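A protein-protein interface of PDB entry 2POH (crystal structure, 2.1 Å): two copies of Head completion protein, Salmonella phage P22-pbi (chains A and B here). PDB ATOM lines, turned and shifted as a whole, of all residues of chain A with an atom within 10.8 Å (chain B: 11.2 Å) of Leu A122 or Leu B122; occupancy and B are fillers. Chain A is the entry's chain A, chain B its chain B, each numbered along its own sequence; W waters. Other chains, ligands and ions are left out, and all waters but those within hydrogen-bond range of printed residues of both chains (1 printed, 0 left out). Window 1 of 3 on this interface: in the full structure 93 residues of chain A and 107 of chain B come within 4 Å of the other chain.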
ATOM      1  N   SER A 114       0.306  22.250 -33.803  1.00  0.00           N
ATOM      2  CA  SER A 114       0.894  21.845 -32.539  1.00  0.00           C
ATOM      3  C   SER A 114       2.246  21.162 -32.747  1.00  0.00           C
ATOM      4  O   SER A 114       3.231  21.439 -32.058  1.00  0.00           O
ATOM      5  CB  SER A 114      -0.066  20.900 -31.806  1.00  0.00           C
ATOM      6  OG  SER A 114      -1.040  21.593 -31.056  1.00  0.00           O
ATOM      7  N   LEU A 115       2.291  20.258 -33.722  1.00  0.00           N
ATOM      8  CA  LEU A 115       3.499  19.497 -34.026  1.00  0.00           C
ATOM      9  C   LEU A 115       4.601  20.360 -34.637  1.00  0.00           C
ATOM     10  O   LEU A 115       5.783  20.186 -34.306  1.00  0.00           O
ATOM     11  CB  LEU A 115       3.150  18.306 -34.933  1.00  0.00           C
ATOM     12  CG  LEU A 115       2.067  17.389 -34.342  1.00  0.00           C
ATOM     13  CD1 LEU A 115       1.485  16.438 -35.377  1.00  0.00           C
ATOM     14  CD2 LEU A 115       2.637  16.617 -33.158  1.00  0.00           C
ATOM     15  N   GLN A 116       4.241  21.305 -35.524  1.00  0.00           N
ATOM     16  CA  GLN A 116       5.305  22.153 -36.066  1.00  0.00           C
ATOM     17  C   GLN A 116       5.938  22.992 -34.957  1.00  0.00           C
ATOM     18  O   GLN A 116       7.156  23.160 -34.898  1.00  0.00           O
ATOM     19  CB  GLN A 116       4.803  23.059 -37.176  1.00  0.00           C
ATOM     20  CG  GLN A 116       4.462  22.367 -38.492  1.00  0.00           C
ATOM     21  CD  GLN A 116       3.318  23.114 -39.162  1.00  0.00           C
ATOM     22  OE1 GLN A 116       3.064  23.001 -40.361  1.00  0.00           O
ATOM     23  NE2 GLN A 116       2.627  23.899 -38.338  1.00  0.00           N
ATOM     24  N   THR A 117       5.119  23.524 -34.060  1.00  0.00           N
ATOM     25  CA  THR A 117       5.660  24.250 -32.904  1.00  0.00           C
ATOM     26  C   THR A 117       6.639  23.372 -32.136  1.00  0.00           C
ATOM     27  O   THR A 117       7.846  23.616 -32.065  1.00  0.00           O
ATOM     28  CB  THR A 117       4.516  24.737 -31.996  1.00  0.00           C
ATOM     29  OG1 THR A 117       3.775  25.784 -32.645  1.00  0.00           O
ATOM     30  CG2 THR A 117       5.070  25.334 -30.708  1.00  0.00           C
ATOM     31  N   ASN A 118       6.142  22.290 -31.538  1.00  0.00           N
ATOM     32  CA  ASN A 118       7.004  21.399 -30.766  1.00  0.00           C
ATOM     33  C   ASN A 118       8.229  20.899 -31.512  1.00  0.00           C
ATOM     34  O   ASN A 118       9.295  20.648 -30.926  1.00  0.00           O
ATOM     35  CB  ASN A 118       6.166  20.196 -30.300  1.00  0.00           C
ATOM     36  CG  ASN A 118       5.195  20.616 -29.214  1.00  0.00           C
ATOM     37  OD1 ASN A 118       5.207  21.771 -28.779  1.00  0.00           O
ATOM     38  ND2 ASN A 118       4.360  19.680 -28.783  1.00  0.00           N
ATOM     39  N   VAL A 119       8.110  20.718 -32.830  1.00  0.00           N
ATOM     40  CA  VAL A 119       9.291  20.237 -33.549  1.00  0.00           C
ATOM     41  C   VAL A 119      10.278  21.388 -33.707  1.00  0.00           C
ATOM     42  O   VAL A 119      11.496  21.223 -33.648  1.00  0.00           O
ATOM     43  CB  VAL A 119       8.949  19.626 -34.915  1.00  0.00           C
ATOM     44  CG1 VAL A 119      10.017  19.963 -35.942  1.00  0.00           C
ATOM     45  CG2 VAL A 119       8.796  18.117 -34.772  1.00  0.00           C
ATOM     46  N   SER A 120       9.719  22.581 -33.900  1.00  0.00           N
ATOM     47  CA  SER A 120      10.569  23.765 -33.946  1.00  0.00           C
ATOM     48  C   SER A 120      11.325  23.939 -32.635  1.00  0.00           C
ATOM     49  O   SER A 120      12.536  24.167 -32.599  1.00  0.00           O
ATOM     50  CB  SER A 120       9.712  24.998 -34.215  1.00  0.00           C
ATOM     51  OG  SER A 120       8.957  24.832 -35.400  1.00  0.00           O
ATOM     52  N   ALA A 121      10.572  23.825 -31.550  1.00  0.00           N
ATOM     53  CA  ALA A 121      11.103  23.873 -30.201  1.00  0.00           C
ATOM     54  C   ALA A 121      12.076  22.722 -29.941  1.00  0.00           C
ATOM     55  O   ALA A 121      12.966  22.899 -29.102  1.00  0.00           O
ATOM     56  CB  ALA A 121       9.972  23.830 -29.183  1.00  0.00           C
ATOM     57  N   LEU A 122      11.889  21.611 -30.646  1.00  0.00           N
ATOM     58  CA  LEU A 122      12.750  20.445 -30.551  1.00  0.00           C
ATOM     59  C   LEU A 122      14.106  20.738 -31.194  1.00  0.00           C
ATOM     60  O   LEU A 122      15.149  20.449 -30.585  1.00  0.00           O
ATOM     61  CB  LEU A 122      12.124  19.219 -31.201  1.00  0.00           C
ATOM     62  CG  LEU A 122      11.194  18.338 -30.363  1.00  0.00           C
ATOM     63  CD1 LEU A 122      10.939  17.013 -31.071  1.00  0.00           C
ATOM     64  CD2 LEU A 122      11.754  18.093 -28.973  1.00  0.00           C
ATOM     65  N   ASP A 123      14.081  21.304 -32.400  1.00  0.00           N
ATOM     66  CA  ASP A 123      15.332  21.679 -33.061  1.00  0.00           C
ATOM     67  C   ASP A 123      16.158  22.558 -32.121  1.00  0.00           C
ATOM     68  O   ASP A 123      17.346  22.310 -31.905  1.00  0.00           O
ATOM     69  CB  ASP A 123      15.076  22.411 -34.371  1.00  0.00           C
ATOM     70  CG  ASP A 123      16.210  23.314 -34.816  1.00  0.00           C
ATOM     71  OD1 ASP A 123      16.441  24.386 -34.212  1.00  0.00           O
ATOM     72  OD2 ASP A 123      16.882  22.951 -35.808  1.00  0.00           O
ATOM     73  N   GLY A 124      15.479  23.572 -31.594  1.00  0.00           N
ATOM     74  CA  GLY A 124      16.073  24.501 -30.656  1.00  0.00           C
ATOM     75  C   GLY A 124      16.881  23.831 -29.563  1.00  0.00           C
ATOM     76  O   GLY A 124      18.025  24.219 -29.309  1.00  0.00           O
ATOM     77  N   ARG A 125      16.309  22.835 -28.905  1.00  0.00           N
ATOM     78  CA  ARG A 125      16.906  22.188 -27.745  1.00  0.00           C
ATOM     79  C   ARG A 125      18.065  21.274 -28.113  1.00  0.00           C
ATOM     80  O   ARG A 125      18.999  21.089 -27.336  1.00  0.00           O
ATOM     81  CB  ARG A 125      15.821  21.383 -27.014  1.00  0.00           C
ATOM     82  CG  ARG A 125      14.728  22.242 -26.393  1.00  0.00           C
ATOM     83  CD  ARG A 125      14.176  21.610 -25.124  1.00  0.00           C
ATOM     84  NE  ARG A 125      13.802  20.222 -25.336  1.00  0.00           N
ATOM     85  CZ  ARG A 125      13.519  19.316 -24.424  1.00  0.00           C
ATOM     86  NH1 ARG A 125      13.540  19.573 -23.128  1.00  0.00           N
ATOM     87  NH2 ARG A 125      13.197  18.088 -24.827  1.00  0.00           N
ATOM     88  N   VAL A 126      17.984  20.700 -29.303  1.00  0.00           N
ATOM     89  CA  VAL A 126      18.929  19.776 -29.893  1.00  0.00           C
ATOM     90  C   VAL A 126      20.149  20.514 -30.433  1.00  0.00           C
ATOM     91  O   VAL A 126      21.275  20.054 -30.255  1.00  0.00           O
ATOM     92  CB  VAL A 126      18.289  18.971 -31.037  1.00  0.00           C
ATOM     93  CG1 VAL A 126      19.249  17.918 -31.565  1.00  0.00           C
ATOM     94  CG2 VAL A 126      16.985  18.339 -30.565  1.00  0.00           C
ATOM     95  N   THR A 127      19.907  21.652 -31.084  1.00  0.00           N
ATOM     96  CA  THR A 127      21.051  22.444 -31.537  1.00  0.00           C
ATOM     97  C   THR A 127      21.928  22.797 -30.333  1.00  0.00           C
ATOM     98  O   THR A 127      23.141  22.582 -30.362  1.00  0.00           O
ATOM     99  CB  THR A 127      20.656  23.735 -32.259  1.00  0.00           C
ATOM    100  OG1 THR A 127      19.946  23.423 -33.468  1.00  0.00           O
ATOM    101  CG2 THR A 127      21.909  24.507 -32.669  1.00  0.00           C
ATOM    102  N   THR A 128      21.283  23.320 -29.299  1.00  0.00           N
ATOM    103  CA  THR A 128      21.930  23.736 -28.060  1.00  0.00           C
ATOM    104  C   THR A 128      22.641  22.593 -27.345  1.00  0.00           C
ATOM    105  O   THR A 128      23.651  22.776 -26.645  1.00  0.00           O
ATOM    106  CB  THR A 128      20.889  24.355 -27.101  1.00  0.00           C
ATOM    107  OG1 THR A 128      20.414  25.585 -27.656  1.00  0.00           O
ATOM    108  CG2 THR A 128      21.515  24.683 -25.753  1.00  0.00           C
ATOM    109  N   ALA A 129      22.115  21.385 -27.507  1.00  0.00           N
ATOM    110  CA  ALA A 129      22.716  20.211 -26.877  1.00  0.00           C
ATOM    111  C   ALA A 129      23.948  19.773 -27.657  1.00  0.00           C
ATOM    112  O   ALA A 129      25.006  19.535 -27.073  1.00  0.00           O
ATOM    113  CB  ALA A 129      21.664  19.120 -26.754  1.00  0.00           C
ATOM    114  N   GLU A 130      23.845  19.683 -28.984  1.00  0.00           N
ATOM    115  CA  GLU A 130      25.011  19.408 -29.814  1.00  0.00           C
ATOM    116  C   GLU A 130      26.122  20.416 -29.514  1.00  0.00           C
ATOM    117  O   GLU A 130      27.302  20.096 -29.464  1.00  0.00           O
ATOM    118  CB  GLU A 130      24.690  19.475 -31.304  1.00  0.00           C
ATOM    119  CG  GLU A 130      23.367  18.898 -31.752  1.00  0.00           C
ATOM    120  CD  GLU A 130      23.102  19.004 -33.242  1.00  0.00           C
ATOM    121  OE1 GLU A 130      23.277  20.096 -33.824  1.00  0.00           O
ATOM    122  OE2 GLU A 130      22.709  17.995 -33.866  1.00  0.00           O
ATOM    123  N   ASN A 131      25.726  21.671 -29.322  1.00  0.00           N
ATOM    124  CA  ASN A 131      26.672  22.762 -29.154  1.00  0.00           C
ATOM    125  C   ASN A 131      27.416  22.656 -27.837  1.00  0.00           C
ATOM    126  O   ASN A 131      28.652  22.716 -27.815  1.00  0.00           O
ATOM    127  CB  ASN A 131      25.973  24.120 -29.236  1.00  0.00           C
ATOM    128  CG  ASN A 131      25.872  24.646 -30.652  1.00  0.00           C
ATOM    129  OD1 ASN A 131      26.195  23.925 -31.601  1.00  0.00           O
ATOM    130  ND2 ASN A 131      25.425  25.891 -30.798  1.00  0.00           N
ATOM    131  N   SER B 114       1.031   8.872 -35.718  1.00  0.00           N
ATOM    132  CA  SER B 114       2.312   8.169 -35.691  1.00  0.00           C
ATOM    133  C   SER B 114       3.443   9.124 -35.326  1.00  0.00           C
ATOM    134  O   SER B 114       4.417   8.786 -34.651  1.00  0.00           O
ATOM    135  CB  SER B 114       2.589   7.532 -37.052  1.00  0.00           C
ATOM    136  OG  SER B 114       2.865   6.148 -36.935  1.00  0.00           O
ATOM    137  N   LEU B 115       3.282  10.351 -35.812  1.00  0.00           N
ATOM    138  CA  LEU B 115       4.216  11.433 -35.538  1.00  0.00           C
ATOM    139  C   LEU B 115       4.203  11.779 -34.050  1.00  0.00           C
ATOM    140  O   LEU B 115       5.239  11.774 -33.395  1.00  0.00           O
ATOM    141  CB  LEU B 115       3.862  12.658 -36.388  1.00  0.00           C
ATOM    142  CG  LEU B 115       4.428  12.655 -37.812  1.00  0.00           C
ATOM    143  CD1 LEU B 115       3.627  13.563 -38.733  1.00  0.00           C
ATOM    144  CD2 LEU B 115       5.896  13.064 -37.802  1.00  0.00           C
ATOM    145  N   GLN B 116       3.012  12.061 -33.544  1.00  0.00           N
ATOM    146  CA  GLN B 116       2.761  12.483 -32.173  1.00  0.00           C
ATOM    147  C   GLN B 116       3.488  11.599 -31.173  1.00  0.00           C
ATOM    148  O   GLN B 116       4.072  12.039 -30.180  1.00  0.00           O
ATOM    149  CB  GLN B 116       1.246  12.464 -31.916  1.00  0.00           C
ATOM    150  CG  GLN B 116       0.499  13.545 -32.688  1.00  0.00           C
ATOM    151  CD  GLN B 116      -1.001  13.455 -32.493  1.00  0.00           C
ATOM    152  OE1 GLN B 116      -1.499  12.439 -31.991  1.00  0.00           O
ATOM    153  NE2 GLN B 116      -1.738  14.492 -32.887  1.00  0.00           N
ATOM    154  N   THR B 117       3.426  10.310 -31.481  1.00  0.00           N
ATOM    155  CA  THR B 117       4.086   9.268 -30.719  1.00  0.00           C
ATOM    156  C   THR B 117       5.597   9.486 -30.711  1.00  0.00           C
ATOM    157  O   THR B 117       6.261   9.457 -29.675  1.00  0.00           O
ATOM    158  CB  THR B 117       3.772   7.882 -31.315  1.00  0.00           C
ATOM    159  OG1 THR B 117       2.391   7.577 -31.064  1.00  0.00           O
ATOM    160  CG2 THR B 117       4.626   6.808 -30.656  1.00  0.00           C
ATOM    161  N   ASN B 118       6.109   9.715 -31.918  1.00  0.00           N
ATOM    162  CA  ASN B 118       7.530   9.916 -32.146  1.00  0.00           C
ATOM    163  C   ASN B 118       8.027  11.282 -31.696  1.00  0.00           C
ATOM    164  O   ASN B 118       9.231  11.439 -31.464  1.00  0.00           O
ATOM    165  CB  ASN B 118       7.864   9.694 -33.632  1.00  0.00           C
ATOM    166  CG  ASN B 118       8.942   8.630 -33.782  1.00  0.00           C
ATOM    167  OD1 ASN B 118       8.880   7.590 -33.130  1.00  0.00           O
ATOM    168  ND2 ASN B 118       9.937   8.880 -34.627  1.00  0.00           N
ATOM    169  N   VAL B 119       7.168  12.292 -31.554  1.00  0.00           N
ATOM    170  CA  VAL B 119       7.690  13.573 -31.079  1.00  0.00           C
ATOM    171  C   VAL B 119       7.670  13.625 -29.554  1.00  0.00           C
ATOM    172  O   VAL B 119       8.536  14.227 -28.920  1.00  0.00           O
ATOM    173  CB  VAL B 119       6.911  14.786 -31.609  1.00  0.00           C
ATOM    174  CG1 VAL B 119       7.208  15.993 -30.720  1.00  0.00           C
ATOM    175  CG2 VAL B 119       7.254  15.088 -33.055  1.00  0.00           C
ATOM    176  N   SER B 120       6.667  12.990 -28.937  1.00  0.00           N
ATOM    177  CA  SER B 120       6.657  13.003 -27.480  1.00  0.00           C
ATOM    178  C   SER B 120       7.899  12.267 -26.972  1.00  0.00           C
ATOM    179  O   SER B 120       8.585  12.742 -26.078  1.00  0.00           O
ATOM    180  CB  SER B 120       5.438  12.325 -26.862  1.00  0.00           C
ATOM    181  OG  SER B 120       5.870  11.712 -25.642  1.00  0.00           O
ATOM    182  N   ALA B 121       8.109  11.120 -27.595  1.00  0.00           N
ATOM    183  CA  ALA B 121       9.270  10.273 -27.340  1.00  0.00           C
ATOM    184  C   ALA B 121      10.563  11.075 -27.487  1.00  0.00           C
ATOM    185  O   ALA B 121      11.488  10.892 -26.697  1.00  0.00           O
ATOM    186  CB  ALA B 121       9.250   9.068 -28.264  1.00  0.00           C
ATOM    187  N   LEU B 122      10.586  11.946 -28.493  1.00  0.00           N
ATOM    188  CA  LEU B 122      11.735  12.807 -28.764  1.00  0.00           C
ATOM    189  C   LEU B 122      11.974  13.747 -27.583  1.00  0.00           C
ATOM    190  O   LEU B 122      13.095  13.926 -27.129  1.00  0.00           O
ATOM    191  CB  LEU B 122      11.525  13.629 -30.032  1.00  0.00           C
ATOM    192  CG  LEU B 122      12.522  13.480 -31.178  1.00  0.00           C
ATOM    193  CD1 LEU B 122      13.667  12.552 -30.804  1.00  0.00           C
ATOM    194  CD2 LEU B 122      11.801  12.995 -32.433  1.00  0.00           C
ATOM    195  N   ASP B 123      10.869  14.329 -27.126  1.00  0.00           N
ATOM    196  CA  ASP B 123      10.875  15.197 -25.957  1.00  0.00           C
ATOM    197  C   ASP B 123      11.672  14.583 -24.806  1.00  0.00           C
ATOM    198  O   ASP B 123      12.475  15.251 -24.148  1.00  0.00           O
ATOM    199  CB  ASP B 123       9.436  15.475 -25.524  1.00  0.00           C
ATOM    200  CG  ASP B 123       8.788  16.600 -26.308  1.00  0.00           C
ATOM    201  OD1 ASP B 123       8.810  16.564 -27.558  1.00  0.00           O
ATOM    202  OD2 ASP B 123       8.251  17.530 -25.668  1.00  0.00           O
ATOM    203  N   GLY B 124      11.445  13.300 -24.568  1.00  0.00           N
ATOM    204  CA  GLY B 124      11.989  12.555 -23.458  1.00  0.00           C
ATOM    205  C   GLY B 124      13.485  12.335 -23.521  1.00  0.00           C
ATOM    206  O   GLY B 124      14.174  12.533 -22.515  1.00  0.00           O
ATOM    207  N   ARG B 125      13.957  11.932 -24.699  1.00  0.00           N
ATOM    208  CA  ARG B 125      15.371  11.688 -24.954  1.00  0.00           C
ATOM    209  C   ARG B 125      16.110  13.014 -25.017  1.00  0.00           C
ATOM    210  O   ARG B 125      17.332  13.114 -24.879  1.00  0.00           O
ATOM    211  CB  ARG B 125      15.561  10.885 -26.242  1.00  0.00           C
ATOM    212  CG  ARG B 125      15.004   9.474 -26.217  1.00  0.00           C
ATOM    213  CD  ARG B 125      15.442   8.643 -27.408  1.00  0.00           C
ATOM    214  NE  ARG B 125      16.584   9.238 -28.100  1.00  0.00           N
ATOM    215  CZ  ARG B 125      16.935   9.010 -29.356  1.00  0.00           C
ATOM    216  NH1 ARG B 125      16.253   8.178 -30.137  1.00  0.00           N
ATOM    217  NH2 ARG B 125      17.993   9.622 -29.857  1.00  0.00           N
ATOM    218  N   VAL B 126      15.348  14.100 -25.219  1.00  0.00           N
ATOM    219  CA  VAL B 126      16.083  15.382 -25.195  1.00  0.00           C
ATOM    220  C   VAL B 126      16.265  15.847 -23.756  1.00  0.00           C
ATOM    221  O   VAL B 126      17.312  16.330 -23.334  1.00  0.00           O
ATOM    222  CB  VAL B 126      15.366  16.422 -26.059  1.00  0.00           C
ATOM    223  CG1 VAL B 126      16.011  17.794 -25.965  1.00  0.00           C
ATOM    224  CG2 VAL B 126      15.356  15.959 -27.512  1.00  0.00           C
ATOM    225  N   THR B 127      15.214  15.680 -22.970  1.00  0.00           N
ATOM    226  CA  THR B 127      15.175  15.968 -21.548  1.00  0.00           C
ATOM    227  C   THR B 127      16.264  15.243 -20.758  1.00  0.00           C
ATOM    228  O   THR B 127      16.924  15.850 -19.908  1.00  0.00           O
ATOM    229  CB  THR B 127      13.797  15.561 -20.983  1.00  0.00           C
ATOM    230  OG1 THR B 127      12.812  16.535 -21.355  1.00  0.00           O
ATOM    231  CG2 THR B 127      13.849  15.506 -19.468  1.00  0.00           C
ATOM    232  N   THR B 128      16.448  13.955 -21.017  1.00  0.00           N
ATOM    233  CA  THR B 128      17.429  13.086 -20.384  1.00  0.00           C
ATOM    234  C   THR B 128      18.866  13.521 -20.675  1.00  0.00           C
ATOM    235  O   THR B 128      19.704  13.658 -19.775  1.00  0.00           O
ATOM    236  CB  THR B 128      17.250  11.644 -20.899  1.00  0.00           C
ATOM    237  OG1 THR B 128      15.864  11.289 -20.783  1.00  0.00           O
ATOM    238  CG2 THR B 128      18.057  10.648 -20.079  1.00  0.00           C
ATOM    239  N   ALA B 129      19.106  13.717 -21.969  1.00  0.00           N
ATOM    240  CA  ALA B 129      20.366  14.191 -22.513  1.00  0.00           C
ATOM    241  C   ALA B 129      20.696  15.562 -21.916  1.00  0.00           C
ATOM    242  O   ALA B 129      21.801  15.727 -21.387  1.00  0.00           O
ATOM    243  CB  ALA B 129      20.322  14.282 -24.029  1.00  0.00           C
ATOM    244  N   GLU B 130      19.709  16.456 -22.031  1.00  0.00           N
ATOM    245  CA  GLU B 130      19.794  17.796 -21.453  1.00  0.00           C
ATOM    246  C   GLU B 130      20.230  17.672 -19.997  1.00  0.00           C
ATOM    247  O   GLU B 130      21.077  18.420 -19.501  1.00  0.00           O
ATOM    248  CB  GLU B 130      18.475  18.551 -21.550  1.00  0.00           C
ATOM    249  CG  GLU B 130      18.290  19.469 -22.739  1.00  0.00           C
ATOM    250  CD  GLU B 130      16.845  19.743 -23.122  1.00  0.00           C
ATOM    251  OE1 GLU B 130      16.607  20.444 -24.136  1.00  0.00           O
ATOM    252  OE2 GLU B 130      15.917  19.272 -22.428  1.00  0.00           O
ATOM    253  N   ASN B 131      19.661  16.698 -19.276  1.00  0.00           N
ATOM    254  CA  ASN B 131      20.089  16.540 -17.885  1.00  0.00           C
ATOM    255  C   ASN B 131      21.455  15.869 -17.795  1.00  0.00           C
ATOM    256  O   ASN B 131      22.280  16.234 -16.962  1.00  0.00           O
ATOM    257  CB  ASN B 131      19.082  15.723 -17.078  1.00  0.00           C
ATOM    258  CG  ASN B 131      17.706  16.346 -17.029  1.00  0.00           C
ATOM    259  OD1 ASN B 131      16.706  15.656 -17.245  1.00  0.00           O
ATOM    260  ND2 ASN B 131      17.647  17.642 -16.748  1.00  0.00           N
HETATM  261  O   HOH W   1      19.323  21.818 -24.548  1.00  0.00           O
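The guanidinium group (NH2) of Arg A125 sits at hydrogen-bond distance from the backbone carbonyl oxygen (O) of Asp B123. The guanidinium group of Arg A125 is in salt-bridge range of the side-chain carboxylate of Glu B130 (2.5 Å).
O of Val B119 lies close to OD1 of Asp B123, at 2.7 Å. The backbone carbonyl oxygen (O) of Asp B123 sits at hydrogen-bond distance from the side-chain hydroxyl (OG1) of Thr B127 (3.1 Å). O of Thr B127 lies close to OD1 of Asn B131, 2.7 Å away.
Among the printed residues, pairs that only touch across the chains: Arg A125 with Val B126 (3.0 Å), Leu A122 with Leu B122 (3.6 Å), Arg A125 with Thr B127 (3.6 Å), Leu A122 with Asp B123 (3.6 Å), Leu A115 with Gln B116 (3.8 Å), Val A119 with Val B119 (3.8 Å) and Leu A122 with Val B119 (3.9 Å).
Of the printed residues of chain B, Leu A115 touches Gln B116 (3.8 Å). No residue of chain B comes within 4 Å of Asn A118. No residue of chain B comes within 4 Å of Ala A121. No residue of chain B comes within 4 Å of Gly A124. Arg A125 touches just these residues of chain B: Asp B123, Val B126, Thr B127 and Glu B130. Printed residues of chain A within 4 Å of Gln B116: Leu A115 (3.8 Å). No residue of chain A comes within 4 Å of Asn B118. Val B119 touches just these residues of chain A: Val A119 (3.8 Å) and Leu A122 (3.9 Å). No residue of chain A comes within 4 Å of Ser B120. No residue of chain A comes within 4 Å of Ala B121. Of chain A, only Leu A122 (3.6 Å) comes within 4 Å of Leu B122. Gly B124 touches none of the printed residues of chain A. No residue of chain A comes within 4 Å of Arg B125. Val B126 touches just one residue of chain A: Arg A125. Printed residues of chain A within 4 Å of Glu B130: Arg A125. The nearest residue of chain B that does not touch Leu A122 is Val B126 (4.4 Å).
Of the 18 printed residues of chain B, 7 touch a printed residue of chain A. Hydrophobic or aromatic side chains of chain B that line the printed part of chain A: Val B119, Leu B122 and Val B126. Along chain B the printed residues that touch a printed residue of chain A span positions 116 to 130. Of the 18 printed residues of chain A, 4 touch a printed residue of chain B. Hydrophobic or aromatic side chains of chain A that line the printed part of chain B: Leu A115, Val A119 and Leu A122. Among the printed residues, 9 pairs touch across the chains. Among the printed residues, Asp or Glu carboxylates within 4 Å of a Lys or Arg side-chain nitrogen of the other chain: Arg A125 with Glu B130.
Leu A115 touches Gln B116, but with the chains exchanged Gln A116 does not touch Leu B115 (8.4 Å). Leu A122 touches its own counterpart, Leu B122. Leu A122 touches Asp B123, but with the chains exchanged Asp A123 does not touch Leu B122 (8.1 Å). Arg A125 touches Val B126, but with the chains exchanged Val A126 does not touch Arg B125 (7.7 Å). 18 positions are printed for both chains. Of the 9 pairs that touch across the chains among the printed residues, 2 have their exchanged pair printed and touching as well.
Water W1 bridges the backbone carbonyl oxygen (O) of Arg A125 and the side-chain carboxylate (OE1) of Glu B130.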
